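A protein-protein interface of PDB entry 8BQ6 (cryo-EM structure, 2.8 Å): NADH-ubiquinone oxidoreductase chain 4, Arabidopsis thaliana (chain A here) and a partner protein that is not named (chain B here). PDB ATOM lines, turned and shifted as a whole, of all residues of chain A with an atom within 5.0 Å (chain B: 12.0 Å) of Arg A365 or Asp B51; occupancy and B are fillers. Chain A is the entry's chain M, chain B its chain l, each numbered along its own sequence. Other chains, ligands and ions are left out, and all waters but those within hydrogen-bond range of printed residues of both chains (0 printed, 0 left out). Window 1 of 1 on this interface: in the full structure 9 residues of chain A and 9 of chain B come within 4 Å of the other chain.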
ATOM      1  N   ILE A 302     -33.478 -17.899   7.003  1.00  0.00           N
ATOM      2  CA  ILE A 302     -32.380 -17.135   7.582  1.00  0.00           C
ATOM      3  C   ILE A 302     -31.135 -17.975   7.787  1.00  0.00           C
ATOM      4  O   ILE A 302     -30.099 -17.440   8.210  1.00  0.00           O
ATOM      5  CB  ILE A 302     -32.810 -16.478   8.906  1.00  0.00           C
ATOM      6  CG1 ILE A 302     -33.271 -17.553   9.890  1.00  0.00           C
ATOM      7  CG2 ILE A 302     -33.930 -15.486   8.656  1.00  0.00           C
ATOM      8  CD1 ILE A 302     -33.655 -17.027  11.239  1.00  0.00           C
ATOM      9  N   LEU A 363     -26.173 -18.879  10.299  1.00  0.00           N
ATOM     10  CA  LEU A 363     -27.100 -17.754  10.303  1.00  0.00           C
ATOM     11  C   LEU A 363     -26.551 -16.626   9.435  1.00  0.00           C
ATOM     12  O   LEU A 363     -25.416 -16.180   9.629  1.00  0.00           O
ATOM     13  CB  LEU A 363     -27.337 -17.276  11.734  1.00  0.00           C
ATOM     14  CG  LEU A 363     -28.223 -18.193  12.582  1.00  0.00           C
ATOM     15  CD1 LEU A 363     -28.613 -17.532  13.887  1.00  0.00           C
ATOM     16  CD2 LEU A 363     -29.459 -18.602  11.809  1.00  0.00           C
ATOM     17  N   VAL A 364     -27.369 -16.159   8.487  1.00  0.00           N
ATOM     18  CA  VAL A 364     -26.935 -15.139   7.535  1.00  0.00           C
ATOM     19  C   VAL A 364     -26.579 -13.837   8.239  1.00  0.00           C
ATOM     20  O   VAL A 364     -25.708 -13.090   7.777  1.00  0.00           O
ATOM     21  CB  VAL A 364     -28.026 -14.932   6.465  1.00  0.00           C
ATOM     22  CG1 VAL A 364     -27.547 -14.001   5.386  1.00  0.00           C
ATOM     23  CG2 VAL A 364     -28.393 -16.257   5.843  1.00  0.00           C
ATOM     24  N   ARG A 365     -27.218 -13.557   9.377  1.00  0.00           N
ATOM     25  CA  ARG A 365     -27.028 -12.279  10.054  1.00  0.00           C
ATOM     26  C   ARG A 365     -25.587 -12.065  10.504  1.00  0.00           C
ATOM     27  O   ARG A 365     -25.121 -10.921  10.561  1.00  0.00           O
ATOM     28  CB  ARG A 365     -27.964 -12.189  11.255  1.00  0.00           C
ATOM     29  CG  ARG A 365     -28.101 -10.797  11.807  1.00  0.00           C
ATOM     30  CD  ARG A 365     -28.975  -9.945  10.903  1.00  0.00           C
ATOM     31  NE  ARG A 365     -29.063  -8.565  11.367  1.00  0.00           N
ATOM     32  CZ  ARG A 365     -29.614  -8.187  12.513  1.00  0.00           C
ATOM     33  NH1 ARG A 365     -30.175  -9.058  13.335  1.00  0.00           N
ATOM     34  NH2 ARG A 365     -29.604  -6.899  12.842  1.00  0.00           N
ATOM     35  N   TYR A 366     -24.873 -13.139  10.846  1.00  0.00           N
ATOM     36  CA  TYR A 366     -23.501 -12.987  11.319  1.00  0.00           C
ATOM     37  C   TYR A 366     -22.552 -12.595  10.196  1.00  0.00           C
ATOM     38  O   TYR A 366     -21.587 -11.859  10.431  1.00  0.00           O
ATOM     39  CB  TYR A 366     -23.015 -14.281  11.964  1.00  0.00           C
ATOM     40  CG  TYR A 366     -23.626 -14.588  13.307  1.00  0.00           C
ATOM     41  CD1 TYR A 366     -23.595 -13.663  14.340  1.00  0.00           C
ATOM     42  CD2 TYR A 366     -24.224 -15.815  13.544  1.00  0.00           C
ATOM     43  CE1 TYR A 366     -24.148 -13.953  15.571  1.00  0.00           C
ATOM     44  CE2 TYR A 366     -24.779 -16.113  14.764  1.00  0.00           C
ATOM     45  CZ  TYR A 366     -24.738 -15.182  15.775  1.00  0.00           C
ATOM     46  OH  TYR A 366     -25.296 -15.492  16.992  1.00  0.00           O
ATOM     47  N   TYR A 367     -22.795 -13.085   8.985  1.00  0.00           N
ATOM     48  CA  TYR A 367     -21.875 -12.892   7.879  1.00  0.00           C
ATOM     49  C   TYR A 367     -22.095 -11.522   7.244  1.00  0.00           C
ATOM     50  O   TYR A 367     -22.811 -10.667   7.770  1.00  0.00           O
ATOM     51  CB  TYR A 367     -22.038 -14.011   6.853  1.00  0.00           C
ATOM     52  CG  TYR A 367     -21.595 -15.369   7.345  1.00  0.00           C
ATOM     53  CD1 TYR A 367     -20.251 -15.674   7.504  1.00  0.00           C
ATOM     54  CD2 TYR A 367     -22.527 -16.347   7.652  1.00  0.00           C
ATOM     55  CE1 TYR A 367     -19.851 -16.917   7.954  1.00  0.00           C
ATOM     56  CE2 TYR A 367     -22.138 -17.586   8.102  1.00  0.00           C
ATOM     57  CZ  TYR A 367     -20.802 -17.868   8.252  1.00  0.00           C
ATOM     58  OH  TYR A 367     -20.426 -19.110   8.701  1.00  0.00           O
ATOM     59  N   LYS A 442     -18.486  -7.234  10.081  1.00  0.00           N
ATOM     60  CA  LYS A 442     -19.023  -7.036  11.424  1.00  0.00           C
ATOM     61  C   LYS A 442     -18.052  -7.659  12.419  1.00  0.00           C
ATOM     62  O   LYS A 442     -18.237  -8.808  12.847  1.00  0.00           O
ATOM     63  CB  LYS A 442     -20.417  -7.642  11.558  1.00  0.00           C
ATOM     64  CG  LYS A 442     -21.383  -7.168  10.508  1.00  0.00           C
ATOM     65  CD  LYS A 442     -22.445  -8.201  10.226  1.00  0.00           C
ATOM     66  CE  LYS A 442     -23.482  -7.627   9.288  1.00  0.00           C
ATOM     67  NZ  LYS A 442     -24.607  -8.562   9.032  1.00  0.00           N
ATOM     68  N   PHE A 445     -18.847 -10.040  15.489  1.00  0.00           N
ATOM     69  CA  PHE A 445     -19.161 -11.446  15.271  1.00  0.00           C
ATOM     70  C   PHE A 445     -17.985 -12.222  14.696  1.00  0.00           C
ATOM     71  O   PHE A 445     -17.639 -13.293  15.204  1.00  0.00           O
ATOM     72  CB  PHE A 445     -20.363 -11.592  14.333  1.00  0.00           C
ATOM     73  CG  PHE A 445     -21.553 -10.789  14.741  1.00  0.00           C
ATOM     74  CD1 PHE A 445     -21.934 -10.722  16.067  1.00  0.00           C
ATOM     75  CD2 PHE A 445     -22.307 -10.121  13.796  1.00  0.00           C
ATOM     76  CE1 PHE A 445     -23.032  -9.992  16.443  1.00  0.00           C
ATOM     77  CE2 PHE A 445     -23.407  -9.392  14.166  1.00  0.00           C
ATOM     78  CZ  PHE A 445     -23.770  -9.325  15.491  1.00  0.00           C
ATOM     79  N   LYS B  39     -19.534   1.316  13.448  1.00  0.00           N
ATOM     80  CA  LYS B  39     -19.696   0.265  14.452  1.00  0.00           C
ATOM     81  C   LYS B  39     -21.073  -0.348  14.257  1.00  0.00           C
ATOM     82  O   LYS B  39     -22.083   0.297  14.552  1.00  0.00           O
ATOM     83  CB  LYS B  39     -19.527   0.812  15.867  1.00  0.00           C
ATOM     84  CG  LYS B  39     -19.176  -0.260  16.906  1.00  0.00           C
ATOM     85  CD  LYS B  39     -20.435  -0.926  17.453  1.00  0.00           C
ATOM     86  CE  LYS B  39     -20.161  -2.312  18.010  1.00  0.00           C
ATOM     87  NZ  LYS B  39     -21.343  -2.843  18.752  1.00  0.00           N
ATOM     88  N   HIS B  40     -21.110  -1.588  13.776  1.00  0.00           N
ATOM     89  CA  HIS B  40     -22.383  -2.243  13.508  1.00  0.00           C
ATOM     90  C   HIS B  40     -23.118  -2.535  14.810  1.00  0.00           C
ATOM     91  O   HIS B  40     -22.529  -3.030  15.776  1.00  0.00           O
ATOM     92  CB  HIS B  40     -22.153  -3.529  12.715  1.00  0.00           C
ATOM     93  CG  HIS B  40     -21.459  -4.600  13.495  1.00  0.00           C
ATOM     94  ND1 HIS B  40     -22.115  -5.707  13.988  1.00  0.00           N
ATOM     95  CD2 HIS B  40     -20.169  -4.721  13.886  1.00  0.00           C
ATOM     96  CE1 HIS B  40     -21.256  -6.470  14.639  1.00  0.00           C
ATOM     97  NE2 HIS B  40     -20.068  -5.895  14.591  1.00  0.00           N
ATOM     98  N   ILE B  41     -24.415  -2.232  14.833  1.00  0.00           N
ATOM     99  CA  ILE B  41     -25.172  -2.347  16.071  1.00  0.00           C
ATOM    100  C   ILE B  41     -25.425  -3.816  16.374  1.00  0.00           C
ATOM    101  O   ILE B  41     -26.074  -4.529  15.597  1.00  0.00           O
ATOM    102  CB  ILE B  41     -26.491  -1.567  15.991  1.00  0.00           C
ATOM    103  CG1 ILE B  41     -26.335  -0.299  15.146  1.00  0.00           C
ATOM    104  CG2 ILE B  41     -26.959  -1.207  17.397  1.00  0.00           C
ATOM    105  CD1 ILE B  41     -25.317   0.687  15.674  1.00  0.00           C
ATOM    106  N   VAL B  42     -24.904  -4.270  17.506  1.00  0.00           N
ATOM    107  CA  VAL B  42     -25.136  -5.623  17.998  1.00  0.00           C
ATOM    108  C   VAL B  42     -26.431  -5.605  18.804  1.00  0.00           C
ATOM    109  O   VAL B  42     -26.555  -4.783  19.726  1.00  0.00           O
ATOM    110  CB  VAL B  42     -23.960  -6.102  18.857  1.00  0.00           C
ATOM    111  CG1 VAL B  42     -24.375  -7.257  19.731  1.00  0.00           C
ATOM    112  CG2 VAL B  42     -22.775  -6.473  17.983  1.00  0.00           C
ATOM    113  N   PRO B  43     -27.402  -6.468  18.503  1.00  0.00           N
ATOM    114  CA  PRO B  43     -28.690  -6.402  19.205  1.00  0.00           C
ATOM    115  C   PRO B  43     -28.541  -6.560  20.712  1.00  0.00           C
ATOM    116  O   PRO B  43     -27.697  -7.315  21.201  1.00  0.00           O
ATOM    117  CB  PRO B  43     -29.483  -7.565  18.599  1.00  0.00           C
ATOM    118  CG  PRO B  43     -28.851  -7.804  17.275  1.00  0.00           C
ATOM    119  CD  PRO B  43     -27.396  -7.502  17.456  1.00  0.00           C
ATOM    120  N   ASP B  44     -29.371  -5.817  21.446  1.00  0.00           N
ATOM    121  CA  ASP B  44     -29.475  -5.933  22.892  1.00  0.00           C
ATOM    122  C   ASP B  44     -30.902  -6.172  23.358  1.00  0.00           C
ATOM    123  O   ASP B  44     -31.140  -6.247  24.569  1.00  0.00           O
ATOM    124  CB  ASP B  44     -28.927  -4.673  23.574  1.00  0.00           C
ATOM    125  CG  ASP B  44     -29.313  -3.405  22.846  1.00  0.00           C
ATOM    126  OD1 ASP B  44     -30.454  -3.331  22.341  1.00  0.00           O
ATOM    127  OD2 ASP B  44     -28.479  -2.478  22.784  1.00  0.00           O
ATOM    128  N   LYS B  45     -31.826  -6.298  22.401  1.00  0.00           N
ATOM    129  CA  LYS B  45     -33.250  -6.575  22.720  1.00  0.00           C
ATOM    130  C   LYS B  45     -33.686  -7.813  21.928  1.00  0.00           C
ATOM    131  O   LYS B  45     -33.262  -7.942  20.759  1.00  0.00           O
ATOM    132  CB  LYS B  45     -34.112  -5.361  22.362  1.00  0.00           C
ATOM    133  CG  LYS B  45     -33.865  -4.122  23.210  1.00  0.00           C
ATOM    134  CD  LYS B  45     -34.722  -2.943  22.804  1.00  0.00           C
ATOM    135  CE  LYS B  45     -34.491  -1.719  23.665  1.00  0.00           C
ATOM    136  NZ  LYS B  45     -35.326  -0.577  23.228  1.00  0.00           N
ATOM    137  N   PRO B  46     -34.492  -8.730  22.513  1.00  0.00           N
ATOM    138  CA  PRO B  46     -34.981  -9.923  21.806  1.00  0.00           C
ATOM    139  C   PRO B  46     -35.442  -9.623  20.372  1.00  0.00           C
ATOM    140  O   PRO B  46     -36.341  -8.813  20.204  1.00  0.00           O
ATOM    141  CB  PRO B  46     -36.170 -10.354  22.672  1.00  0.00           C
ATOM    142  CG  PRO B  46     -35.737  -9.981  24.069  1.00  0.00           C
ATOM    143  CD  PRO B  46     -34.967  -8.688  23.900  1.00  0.00           C
ATOM    144  N   LEU B  47     -34.827 -10.283  19.384  1.00  0.00           N
ATOM    145  CA  LEU B  47     -35.160 -10.022  17.957  1.00  0.00           C
ATOM    146  C   LEU B  47     -36.560 -10.548  17.632  1.00  0.00           C
ATOM    147  O   LEU B  47     -36.844 -11.719  17.961  1.00  0.00           O
ATOM    148  CB  LEU B  47     -34.115 -10.705  17.073  1.00  0.00           C
ATOM    149  CG  LEU B  47     -32.751 -10.024  17.009  1.00  0.00           C
ATOM    150  CD1 LEU B  47     -31.941 -10.590  15.857  1.00  0.00           C
ATOM    151  CD2 LEU B  47     -32.903  -8.519  16.858  1.00  0.00           C
ATOM    152  N   SER B  48     -37.386  -9.721  16.983  1.00  0.00           N
ATOM    153  CA  SER B  48     -38.759 -10.140  16.594  1.00  0.00           C
ATOM    154  C   SER B  48     -38.756 -10.779  15.200  1.00  0.00           C
ATOM    155  O   SER B  48     -37.685 -10.828  14.564  1.00  0.00           O
ATOM    156  CB  SER B  48     -39.711  -8.972  16.657  1.00  0.00           C
ATOM    157  OG  SER B  48     -39.500  -8.083  15.568  1.00  0.00           O
ATOM    158  N   VAL B  49     -39.927 -11.226  14.731  1.00  0.00           N
ATOM    159  CA  VAL B  49     -40.037 -11.852  13.380  1.00  0.00           C
ATOM    160  C   VAL B  49     -40.029 -10.719  12.345  1.00  0.00           C
ATOM    161  O   VAL B  49     -40.255  -9.550  12.733  1.00  0.00           O
ATOM    162  CB  VAL B  49     -41.295 -12.732  13.250  1.00  0.00           C
ATOM    163  CG1 VAL B  49     -41.284 -13.857  14.272  1.00  0.00           C
ATOM    164  CG2 VAL B  49     -42.577 -11.926  13.364  1.00  0.00           C
ATOM    165  N   ASN B  50     -39.781 -11.052  11.078  1.00  0.00           N
ATOM    166  CA  ASN B  50     -39.783 -10.037   9.987  1.00  0.00           C
ATOM    167  C   ASN B  50     -38.661  -9.035  10.267  1.00  0.00           C
ATOM    168  O   ASN B  50     -38.874  -7.838  10.053  1.00  0.00           O
ATOM    169  CB  ASN B  50     -41.173  -9.418   9.778  1.00  0.00           C
ATOM    170  CG  ASN B  50     -42.296 -10.433   9.831  1.00  0.00           C
ATOM    171  OD1 ASN B  50     -42.108 -11.603   9.504  1.00  0.00           O
ATOM    172  ND2 ASN B  50     -43.471  -9.997  10.253  1.00  0.00           N
ATOM    173  N   ASP B  51     -37.514  -9.532  10.736  1.00  0.00           N
ATOM    174  CA  ASP B  51     -36.348  -8.665  11.034  1.00  0.00           C
ATOM    175  C   ASP B  51     -35.325  -8.826   9.912  1.00  0.00           C
ATOM    176  O   ASP B  51     -34.557  -7.873   9.684  1.00  0.00           O
ATOM    177  CB  ASP B  51     -35.759  -9.000  12.405  1.00  0.00           C
ATOM    178  CG  ASP B  51     -34.736  -7.991  12.893  1.00  0.00           C
ATOM    179  OD1 ASP B  51     -35.005  -6.777  12.778  1.00  0.00           O
ATOM    180  OD2 ASP B  51     -33.673  -8.426  13.371  1.00  0.00           O
ATOM    181  N   GLU B  52     -35.323  -9.980   9.231  1.00  0.00           N
ATOM    182  CA  GLU B  52     -34.419 -10.130   8.098  1.00  0.00           C
ATOM    183  C   GLU B  52     -34.691  -9.104   7.008  1.00  0.00           C
ATOM    184  O   GLU B  52     -33.827  -8.883   6.155  1.00  0.00           O
ATOM    185  CB  GLU B  52     -34.550 -11.522   7.494  1.00  0.00           C
ATOM    186  CG  GLU B  52     -35.928 -11.757   6.926  1.00  0.00           C
ATOM    187  CD  GLU B  52     -36.727 -12.747   7.723  1.00  0.00           C
ATOM    188  OE1 GLU B  52     -36.953 -12.505   8.926  1.00  0.00           O
ATOM    189  OE2 GLU B  52     -37.160 -13.759   7.136  1.00  0.00           O
ATOM    190  N   LEU B  53     -35.878  -8.492   7.003  1.00  0.00           N
ATOM    191  CA  LEU B  53     -36.260  -7.535   5.975  1.00  0.00           C
ATOM    192  C   LEU B  53     -36.438  -6.120   6.501  1.00  0.00           C
ATOM    193  O   LEU B  53     -37.014  -5.284   5.796  1.00  0.00           O
ATOM    194  CB  LEU B  53     -37.562  -7.975   5.286  1.00  0.00           C
ATOM    195  CG  LEU B  53     -38.824  -8.081   6.147  1.00  0.00           C
ATOM    196  CD1 LEU B  53     -39.466  -6.724   6.385  1.00  0.00           C
ATOM    197  CD2 LEU B  53     -39.810  -9.009   5.485  1.00  0.00           C
ATOM    198  N   MET B  54     -35.966  -5.820   7.706  1.00  0.00           N
ATOM    199  CA  MET B  54     -36.248  -4.520   8.300  1.00  0.00           C
ATOM    200  C   MET B  54     -34.979  -3.787   8.717  1.00  0.00           C
ATOM    201  O   MET B  54     -34.562  -2.835   8.055  1.00  0.00           O
ATOM    202  CB  MET B  54     -37.187  -4.684   9.496  1.00  0.00           C
ATOM    203  CG  MET B  54     -38.659  -4.514   9.141  1.00  0.00           C
ATOM    204  SD  MET B  54     -38.927  -3.389   7.754  1.00  0.00           S
ATOM    205  CE  MET B  54     -39.282  -1.863   8.621  1.00  0.00           C
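Ile A302 touches Glu B52.
Leu B47 touches Arg A365 (CD1 to NH1, 3.4 Å).
Lys A442 touches His B40 (CB to CE1, 3.4 Å).
Phe A445 touches His B40.
Val B42 touches Phe A445 (CG2 to CE1, 3.8 Å).
The side-chain carboxylate (OD2) of Asp B51 is in salt-bridge range of the guanidinium group (NH1) of Arg A365.
No residue of chain B comes within 4 Å of Val A364.
Arg A365 touches just these residues of chain B: Leu B47 and Asp B51.
Of the printed residues of chain B, Lys A442 touches His B40 (3.4 Å).
Printed residues of chain B within 4 Å of Phe A445: His B40 (3.7 Å) and Val B42 (3.8 Å).
Of the printed residues of chain A, Val B42 touches Phe A445 (3.8 Å).
Of the printed residues of chain A, Leu B47 touches Arg A365.
Asp B51 touches just one residue of chain A: Arg A365 (3.6 Å).
Of the printed residues of chain A, Glu B52 touches Ile A302 (3.97 Å).
Met B54 touches none of the printed residues of chain A.
The nearest printed residue of chain A that does not touch Asp B51 is Ile A302 (6.9 Å).
The nearest printed residue of chain A that does not touch Glu B52 is Arg A365 (6.1 Å).
O of Ile A302 is in hydrogen-bond range of N of Val A364, 3.0 Å away.
The backbone carbonyl oxygen (O) of Tyr A367 is in hydrogen-bond range of the side-chain amino group (NZ) of Lys A442 (3.0 Å).
O of Arg A365 sits at hydrogen-bond distance from NZ of Lys A442 (2.9 Å).
Printed residues of chain B that touch a printed residue of chain A: His B40, Val B42, Leu B47, Asp B51 and Glu B52.
Printed residues of chain A that touch a printed residue of chain B: Ile A302, Arg A365, Lys A442 and Phe A445.
Hydrophobic or aromatic side chains of chain A that line the printed part of chain B: Ile A302 and Phe A445.
Among the printed residues, 6 pairs touch across the chains.
Among the printed residues, Asp or Glu carboxylates within 4 Å of a Lys or Arg side-chain nitrogen of the other chain: Arg A365 with Asp B51 (3.6 Å).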
